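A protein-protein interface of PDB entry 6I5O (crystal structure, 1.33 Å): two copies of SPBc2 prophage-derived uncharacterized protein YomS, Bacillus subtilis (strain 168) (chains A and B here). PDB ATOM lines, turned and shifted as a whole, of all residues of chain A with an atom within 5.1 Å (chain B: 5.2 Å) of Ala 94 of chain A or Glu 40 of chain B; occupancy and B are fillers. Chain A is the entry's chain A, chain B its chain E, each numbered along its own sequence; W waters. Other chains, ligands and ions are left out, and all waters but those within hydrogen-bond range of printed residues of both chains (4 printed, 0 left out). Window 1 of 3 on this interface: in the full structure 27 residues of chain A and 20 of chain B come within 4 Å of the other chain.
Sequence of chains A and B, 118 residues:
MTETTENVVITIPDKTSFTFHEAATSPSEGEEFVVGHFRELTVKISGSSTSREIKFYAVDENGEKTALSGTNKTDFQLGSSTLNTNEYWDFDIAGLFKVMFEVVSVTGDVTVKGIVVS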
ATOM      1  N   VAL A  35      17.985  11.459   3.179  1.00  0.00           N
ATOM      2  CA  VAL A  35      18.303  12.572   2.263  1.00  0.00           C
ATOM      3  C   VAL A  35      17.493  13.809   2.593  1.00  0.00           C
ATOM      4  O   VAL A  35      18.042  14.912   2.493  1.00  0.00           O
ATOM      5  CB  VAL A  35      18.111  12.058   0.834  1.00  0.00           C
ATOM      6  CG1 VAL A  35      18.214  13.251  -0.134  1.00  0.00           C
ATOM      7  CG2 VAL A  35      19.156  10.996   0.484  1.00  0.00           C
ATOM      8  N   PHE A  38      17.946  17.478   0.765  1.00  0.00           N
ATOM      9  CA  PHE A  38      19.249  17.709   0.138  1.00  0.00           C
ATOM     10  C   PHE A  38      19.262  17.180  -1.291  1.00  0.00           C
ATOM     11  O   PHE A  38      18.429  16.371  -1.726  1.00  0.00           O
ATOM     12  CB  PHE A  38      20.346  17.107   1.014  1.00  0.00           C
ATOM     13  CG  PHE A  38      20.503  17.868   2.305  1.00  0.00           C
ATOM     14  CD1 PHE A  38      21.113  19.111   2.335  1.00  0.00           C
ATOM     15  CD2 PHE A  38      20.023  17.367   3.505  1.00  0.00           C
ATOM     16  CE1 PHE A  38      21.165  19.839   3.506  1.00  0.00           C
ATOM     17  CE2 PHE A  38      20.064  18.110   4.679  1.00  0.00           C
ATOM     18  CZ  PHE A  38      20.714  19.318   4.695  1.00  0.00           C
ATOM     19  N   ARG A  39      20.214  17.716  -2.056  1.00  0.00           N
ATOM     20  CA  ARG A  39      20.370  17.349  -3.483  1.00  0.00           C
ATOM     21  C   ARG A  39      21.672  16.627  -3.773  1.00  0.00           C
ATOM     22  O   ARG A  39      21.695  15.797  -4.685  1.00  0.00           O
ATOM     23  CB  ARG A  39      20.337  18.584  -4.393  1.00  0.00           C
ATOM     24  CG  ARG A  39      19.062  19.426  -4.369  1.00  0.00           C
ATOM     25  CD  ARG A  39      19.334  20.713  -5.191  1.00  0.00           C
ATOM     26  NE  ARG A  39      18.283  21.707  -5.215  1.00  0.00           N
ATOM     27  CZ  ARG A  39      17.315  21.717  -6.119  1.00  0.00           C
ATOM     28  NH1 ARG A  39      17.188  20.700  -6.930  1.00  0.00           N
ATOM     29  NH2 ARG A  39      16.442  22.699  -6.193  1.00  0.00           N
ATOM     30  N   ASP A  92      24.792  12.587  -6.740  1.00  0.00           N
ATOM     31  CA  ASP A  92      23.483  13.249  -6.909  1.00  0.00           C
ATOM     32  C   ASP A  92      22.446  12.389  -6.196  1.00  0.00           C
ATOM     33  O   ASP A  92      22.219  11.239  -6.604  1.00  0.00           O
ATOM     34  CB  ASP A  92      23.139  13.438  -8.374  1.00  0.00           C
ATOM     35  CG  ASP A  92      21.745  13.998  -8.619  1.00  0.00           C
ATOM     36  OD1 ASP A  92      20.961  14.354  -7.669  1.00  0.00           O
ATOM     37  OD2 ASP A  92      21.405  14.105  -9.827  1.00  0.00           O
ATOM     38  N   ILE A  93      21.920  12.918  -5.099  1.00  0.00           N
ATOM     39  CA  ILE A  93      21.074  12.119  -4.184  1.00  0.00           C
ATOM     40  C   ILE A  93      19.653  12.650  -4.083  1.00  0.00           C
ATOM     41  O   ILE A  93      18.875  12.121  -3.284  1.00  0.00           O
ATOM     42  CB  ILE A  93      21.720  12.070  -2.788  1.00  0.00           C
ATOM     43  CG1 ILE A  93      21.763  13.458  -2.112  1.00  0.00           C
ATOM     44  CG2 ILE A  93      23.079  11.392  -2.816  1.00  0.00           C
ATOM     45  CD1 ILE A  93      22.086  13.444  -0.657  1.00  0.00           C
ATOM     46  N   ALA A  94      19.271  13.636  -4.875  1.00  0.00           N
ATOM     47  CA  ALA A  94      18.031  14.366  -4.633  1.00  0.00           C
ATOM     48  C   ALA A  94      16.807  13.470  -4.632  1.00  0.00           C
ATOM     49  O   ALA A  94      15.851  13.779  -3.914  1.00  0.00           O
ATOM     50  CB  ALA A  94      17.844  15.474  -5.631  1.00  0.00           C
ATOM     51  N   GLY A  95      16.817  12.444  -5.489  1.00  0.00           N
ATOM     52  CA  GLY A  95      15.657  11.556  -5.628  1.00  0.00           C
ATOM     53  C   GLY A  95      15.738  10.269  -4.843  1.00  0.00           C
ATOM     54  O   GLY A  95      14.979   9.318  -5.175  1.00  0.00           O
ATOM     55  N   LEU A  96      16.606  10.212  -3.849  1.00  0.00           N
ATOM     56  CA  LEU A  96      16.833   8.972  -3.075  1.00  0.00           C
ATOM     57  C   LEU A  96      16.266   9.150  -1.681  1.00  0.00           C
ATOM     58  O   LEU A  96      16.296  10.245  -1.139  1.00  0.00           O
ATOM     59  CB  LEU A  96      18.315   8.669  -2.942  1.00  0.00           C
ATOM     60  CG  LEU A  96      19.076   8.534  -4.248  1.00  0.00           C
ATOM     61  CD1 LEU A  96      20.547   8.283  -3.953  1.00  0.00           C
ATOM     62  CD2 LEU A  96      18.503   7.389  -5.109  1.00  0.00           C
ATOM     63  N   LYS B  15       9.931  18.726  -2.863  1.00  0.00           N
ATOM     64  CA  LYS B  15       9.925  17.333  -3.299  1.00  0.00           C
ATOM     65  C   LYS B  15       8.505  16.780  -3.123  1.00  0.00           C
ATOM     66  O   LYS B  15       7.719  17.252  -2.330  1.00  0.00           O
ATOM     67  CB  LYS B  15      10.919  16.492  -2.484  1.00  0.00           C
ATOM     68  CG  LYS B  15      12.355  16.947  -2.664  1.00  0.00           C
ATOM     69  CD  LYS B  15      13.362  16.014  -2.055  1.00  0.00           C
ATOM     70  CE  LYS B  15      14.806  16.461  -2.245  1.00  0.00           C
ATOM     71  NZ  LYS B  15      15.784  15.540  -1.600  1.00  0.00           N
ATOM     72  N   PHE B  38       7.694  20.603 -11.104  1.00  0.00           N
ATOM     73  CA  PHE B  38       8.913  19.855 -10.812  1.00  0.00           C
ATOM     74  C   PHE B  38       9.922  19.836 -11.950  1.00  0.00           C
ATOM     75  O   PHE B  38       9.558  20.137 -13.102  1.00  0.00           O
ATOM     76  CB  PHE B  38       8.534  18.448 -10.334  1.00  0.00           C
ATOM     77  CG  PHE B  38       7.886  18.470  -8.974  1.00  0.00           C
ATOM     78  CD1 PHE B  38       8.647  18.622  -7.826  1.00  0.00           C
ATOM     79  CD2 PHE B  38       6.493  18.470  -8.857  1.00  0.00           C
ATOM     80  CE1 PHE B  38       8.038  18.725  -6.589  1.00  0.00           C
ATOM     81  CE2 PHE B  38       5.883  18.637  -7.622  1.00  0.00           C
ATOM     82  CZ  PHE B  38       6.669  18.720  -6.480  1.00  0.00           C
ATOM     83  N   ARG B  39      11.147  19.499 -11.637  1.00  0.00           N
ATOM     84  CA  ARG B  39      12.251  19.514 -12.634  1.00  0.00           C
ATOM     85  C   ARG B  39      12.817  18.128 -12.898  1.00  0.00           C
ATOM     86  O   ARG B  39      13.231  17.852 -14.028  1.00  0.00           O
ATOM     87  CB  ARG B  39      13.397  20.426 -12.203  1.00  0.00           C
ATOM     88  CG  ARG B  39      13.083  21.905 -12.099  1.00  0.00           C
ATOM     89  CD  ARG B  39      14.337  22.650 -11.473  1.00  0.00           C
ATOM     90  NE  ARG B  39      14.144  24.043 -11.123  1.00  0.00           N
ATOM     91  CZ  ARG B  39      14.318  25.050 -11.989  1.00  0.00           C
ATOM     92  NH1 ARG B  39      14.519  24.743 -13.245  1.00  0.00           N
ATOM     93  NH2 ARG B  39      14.318  26.335 -11.655  1.00  0.00           N
ATOM     94  N   GLU B  40      13.054  17.326 -11.832  1.00  0.00           N
ATOM     95  CA  GLU B  40      13.850  16.072 -11.925  1.00  0.00           C
ATOM     96  C   GLU B  40      13.073  14.964 -11.236  1.00  0.00           C
ATOM     97  O   GLU B  40      12.478  15.224 -10.185  1.00  0.00           O
ATOM     98  CB  GLU B  40      15.192  16.261 -11.211  1.00  0.00           C
ATOM     99  CG  GLU B  40      16.074  15.028 -10.949  1.00  0.00           C
ATOM    100  CD  GLU B  40      17.264  15.359 -10.037  1.00  0.00           C
ATOM    101  OE1 GLU B  40      18.017  16.285 -10.366  1.00  0.00           O
ATOM    102  OE2 GLU B  40      17.333  14.791  -8.956  1.00  0.00           O
ATOM    103  N   LEU B  41      13.116  13.759 -11.787  1.00  0.00           N
ATOM    104  CA  LEU B  41      12.423  12.564 -11.273  1.00  0.00           C
ATOM    105  C   LEU B  41      13.421  11.455 -11.124  1.00  0.00           C
ATOM    106  O   LEU B  41      14.221  11.208 -12.028  1.00  0.00           O
ATOM    107  CB  LEU B  41      11.372  12.145 -12.303  1.00  0.00           C
ATOM    108  CG  LEU B  41      10.709  10.801 -12.098  1.00  0.00           C
ATOM    109  CD1 LEU B  41       9.858  10.757 -10.864  1.00  0.00           C
ATOM    110  CD2 LEU B  41       9.869  10.461 -13.336  1.00  0.00           C
ATOM    111  N   THR B  42      13.348  10.763  -9.994  1.00  0.00           N
ATOM    112  CA  THR B  42      14.094   9.499  -9.827  1.00  0.00           C
ATOM    113  C   THR B  42      13.099   8.394  -9.563  1.00  0.00           C
ATOM    114  O   THR B  42      12.322   8.499  -8.596  1.00  0.00           O
ATOM    115  CB  THR B  42      15.078   9.577  -8.677  1.00  0.00           C
ATOM    116  OG1 THR B  42      16.000  10.655  -8.908  1.00  0.00           O
ATOM    117  CG2 THR B  42      15.834   8.284  -8.493  1.00  0.00           C
ATOM    118  N   PHE B  91      15.522  11.203 -14.509  1.00  0.00           N
ATOM    119  CA  PHE B  91      14.983  11.864 -15.706  1.00  0.00           C
ATOM    120  C   PHE B  91      14.936  13.353 -15.450  1.00  0.00           C
ATOM    121  O   PHE B  91      14.559  13.818 -14.361  1.00  0.00           O
ATOM    122  CB  PHE B  91      13.560  11.398 -15.976  1.00  0.00           C
ATOM    123  CG  PHE B  91      13.445   9.916 -16.192  1.00  0.00           C
ATOM    124  CD1 PHE B  91      13.304   9.062 -15.145  1.00  0.00           C
ATOM    125  CD2 PHE B  91      13.533   9.396 -17.463  1.00  0.00           C
ATOM    126  CE1 PHE B  91      13.249   7.685 -15.323  1.00  0.00           C
ATOM    127  CE2 PHE B  91      13.463   8.016 -17.677  1.00  0.00           C
ATOM    128  CZ  PHE B  91      13.351   7.170 -16.604  1.00  0.00           C
ATOM    129  N   ASP B  92      15.198  14.096 -16.524  1.00  0.00           N
ATOM    130  CA  ASP B  92      14.930  15.549 -16.585  1.00  0.00           C
ATOM    131  C   ASP B  92      13.538  15.723 -17.189  1.00  0.00           C
ATOM    132  O   ASP B  92      13.330  15.358 -18.343  1.00  0.00           O
ATOM    133  CB  ASP B  92      15.979  16.223 -17.448  1.00  0.00           C
ATOM    134  CG  ASP B  92      15.718  17.701 -17.699  1.00  0.00           C
ATOM    135  OD1 ASP B  92      14.729  18.300 -17.147  1.00  0.00           O
ATOM    136  OD2 ASP B  92      16.546  18.264 -18.448  1.00  0.00           O
ATOM    137  N   ILE B  93      12.604  16.183 -16.375  1.00  0.00           N
ATOM    138  CA  ILE B  93      11.169  16.229 -16.729  1.00  0.00           C
ATOM    139  C   ILE B  93      10.632  17.642 -16.780  1.00  0.00           C
ATOM    140  O   ILE B  93       9.399  17.809 -16.954  1.00  0.00           O
ATOM    141  CB  ILE B  93      10.349  15.372 -15.755  1.00  0.00           C
ATOM    142  CG1 ILE B  93      10.389  15.933 -14.327  1.00  0.00           C
ATOM    143  CG2 ILE B  93      10.762  13.915 -15.825  1.00  0.00           C
ATOM    144  CD1 ILE B  93       9.331  15.357 -13.400  1.00  0.00           C
ATOM    145  N   ILE B 115      10.487   9.784  -6.710  1.00  0.00           N
ATOM    146  CA  ILE B 115      10.658  11.006  -5.910  1.00  0.00           C
ATOM    147  C   ILE B 115      10.980  12.094  -6.930  1.00  0.00           C
ATOM    148  O   ILE B 115      11.817  11.906  -7.829  1.00  0.00           O
ATOM    149  CB  ILE B 115      11.790  10.848  -4.900  1.00  0.00           C
ATOM    150  CG1 ILE B 115      11.441   9.784  -3.862  1.00  0.00           C
ATOM    151  CG2 ILE B 115      12.078  12.189  -4.232  1.00  0.00           C
ATOM    152  CD1 ILE B 115      12.499   9.443  -2.858  1.00  0.00           C
ATOM    153  N   VAL B 116      10.295  13.183  -6.783  1.00  0.00           N
ATOM    154  CA  VAL B 116      10.301  14.300  -7.758  1.00  0.00           C
ATOM    155  C   VAL B 116      10.804  15.540  -7.025  1.00  0.00           C
ATOM    156  O   VAL B 116      10.487  15.744  -5.866  1.00  0.00           O
ATOM    157  CB  VAL B 116       8.887  14.583  -8.338  1.00  0.00           C
ATOM    158  CG1 VAL B 116       9.000  15.112  -9.729  1.00  0.00           C
ATOM    159  CG2 VAL B 116       7.993  13.307  -8.331  1.00  0.00           C
ATOM    160  N   VAL B 117      11.614  16.341  -7.730  1.00  0.00           N
ATOM    161  CA  VAL B 117      12.383  17.449  -7.105  1.00  0.00           C
ATOM    162  C   VAL B 117      12.228  18.695  -7.981  1.00  0.00           C
ATOM    163  O   VAL B 117      12.324  18.589  -9.225  1.00  0.00           O
ATOM    164  CB  VAL B 117      13.862  17.047  -6.942  1.00  0.00           C
ATOM    165  CG1 VAL B 117      14.626  18.111  -6.206  1.00  0.00           C
ATOM    166  CG2 VAL B 117      13.973  15.723  -6.228  1.00  0.00           C
HETATM  167  O   HOH W   1      18.817  18.231  -7.707  1.00  0.00           O
HETATM  168  O   HOH W   2      13.418   7.292  -6.138  1.00  0.00           O
HETATM  169  O   HOH W   3      18.517  11.358  -7.392  1.00  0.00           O
HETATM  170  O   HOH W   4      14.810  12.439  -1.657  1.00  0.00           O
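Of the printed residues of chain B, Ala 94 of chain A touches Lys 15, Glu 40 and Val 117.
Of the printed residues of chain B, Leu 96 of chain A touches Ile 115.
Of the printed residues of chain A, Lys 15 of chain B touches Val 35 (3.6 Å), Phe 38 (2.8 Å) and Ala 94 (2.9 Å).
Of the printed residues of chain A, Glu 40 of chain B touches Asp 92 (3.9 Å) and Ala 94 (3.4 Å).
Of the printed residues of chain A, Thr 42 of chain B touches Gly 95 (3.4 Å).
Ile 93 of chain B touches none of the printed residues of chain A.
The nearest printed residue of chain B that does not touch Ala 94 of chain A is Ile 115 of chain B (4.1 Å).
The backbone carbonyl oxygen (O) of Arg 39 of chain A sits at hydrogen-bond distance from the backbone NH (N) of Ile 93 of chain A (2.9 Å).
The backbone carbonyl oxygen of Arg 39 of chain A lies within hydrogen-bond range of the backbone NH of Ala 94 of chain A.
N of Ala 94 of chain A is in hydrogen-bond range of OD1 of Asp 92 of chain A, 3.3 Å away.
The backbone carbonyl oxygen (O) of Val 117 of chain B lies within hydrogen-bond range of the backbone NH (N) of Arg 39 of chain B, 2.8 Å away.
N of Val 117 of chain B lies within hydrogen-bond range of O of Glu 40 of chain B (2.8 Å).
The backbone NH (N) of Thr 42 of chain B sits at hydrogen-bond distance from the backbone carbonyl oxygen (O) of Ile 115 of chain B (2.9 Å).
The backbone carbonyl oxygen (O) of Phe 38 of chain A lies within hydrogen-bond range of the side-chain amino group (NZ) of Lys 15 of chain B (2.8 Å).
The backbone carbonyl oxygen of Ala 94 of chain A is in hydrogen-bond range of the side-chain amino group of Lys 15 of chain B.
Water W4 lies within hydrogen-bond range of the backbone carbonyl oxygen of Leu 96 of chain A (2.7 Å), the backbone carbonyl oxygen of Ala 94 of chain A (2.8 Å) and the side-chain amino group of Lys 15 of chain B (3.3 Å).
Water W2 bridges the backbone carbonyl oxygen of Gly 95 of chain A (2.7 Å) and the backbone carbonyl oxygen of Thr 42 of chain B (2.9 Å).
Water W3 lies within hydrogen-bond range of N of Gly 95 of chain A, OG1 of Thr 42 of chain B and N of Ala 94 of chain A.
Water W1 lies within hydrogen-bond range of the guanidinium group (NH1) of Arg 39 of chain A (3.1 Å) and the side-chain carboxylate (OE1) of Glu 40 of chain B (3.4 Å).
4 positions are printed for both chains.
Of the 10 pairs that touch across the chains among the printed residues, none has its exchanged pair printed and touching as well.
Printed residues of chain B that touch a printed residue of chain A: Lys 15, Glu 40, Thr 42, Ile 115 and Val 117.
Hydrophobic or aromatic side chains of chain B that line the printed part of chain A: Ile 115 and Val 117.
Of the 8 printed residues of chain A, 7 touch a printed residue of chain B.
Printed residues of chain A that touch a printed residue of chain B: Val 35, Phe 38, Arg 39, Asp 92, Ala 94, Gly 95 and Leu 96.
Among the printed residues, 10 pairs touch across the chains.
Among the printed residues, pairs that only touch across the chains: Gly 95 of chain A with Ile 115 of chain B, Gly 95 of chain A with Thr 42 of chain B, Ala 94 of chain A with Glu 40 of chain B, Ala 94 of chain A with Val 117 of chain B, Val 35 of chain A with Lys 15 of chain B, Arg 39 of chain A with Val 117 of chain B, Asp 92 of chain A with Glu 40 of chain B and Leu 96 of chain A with Ile 115 of chain B.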
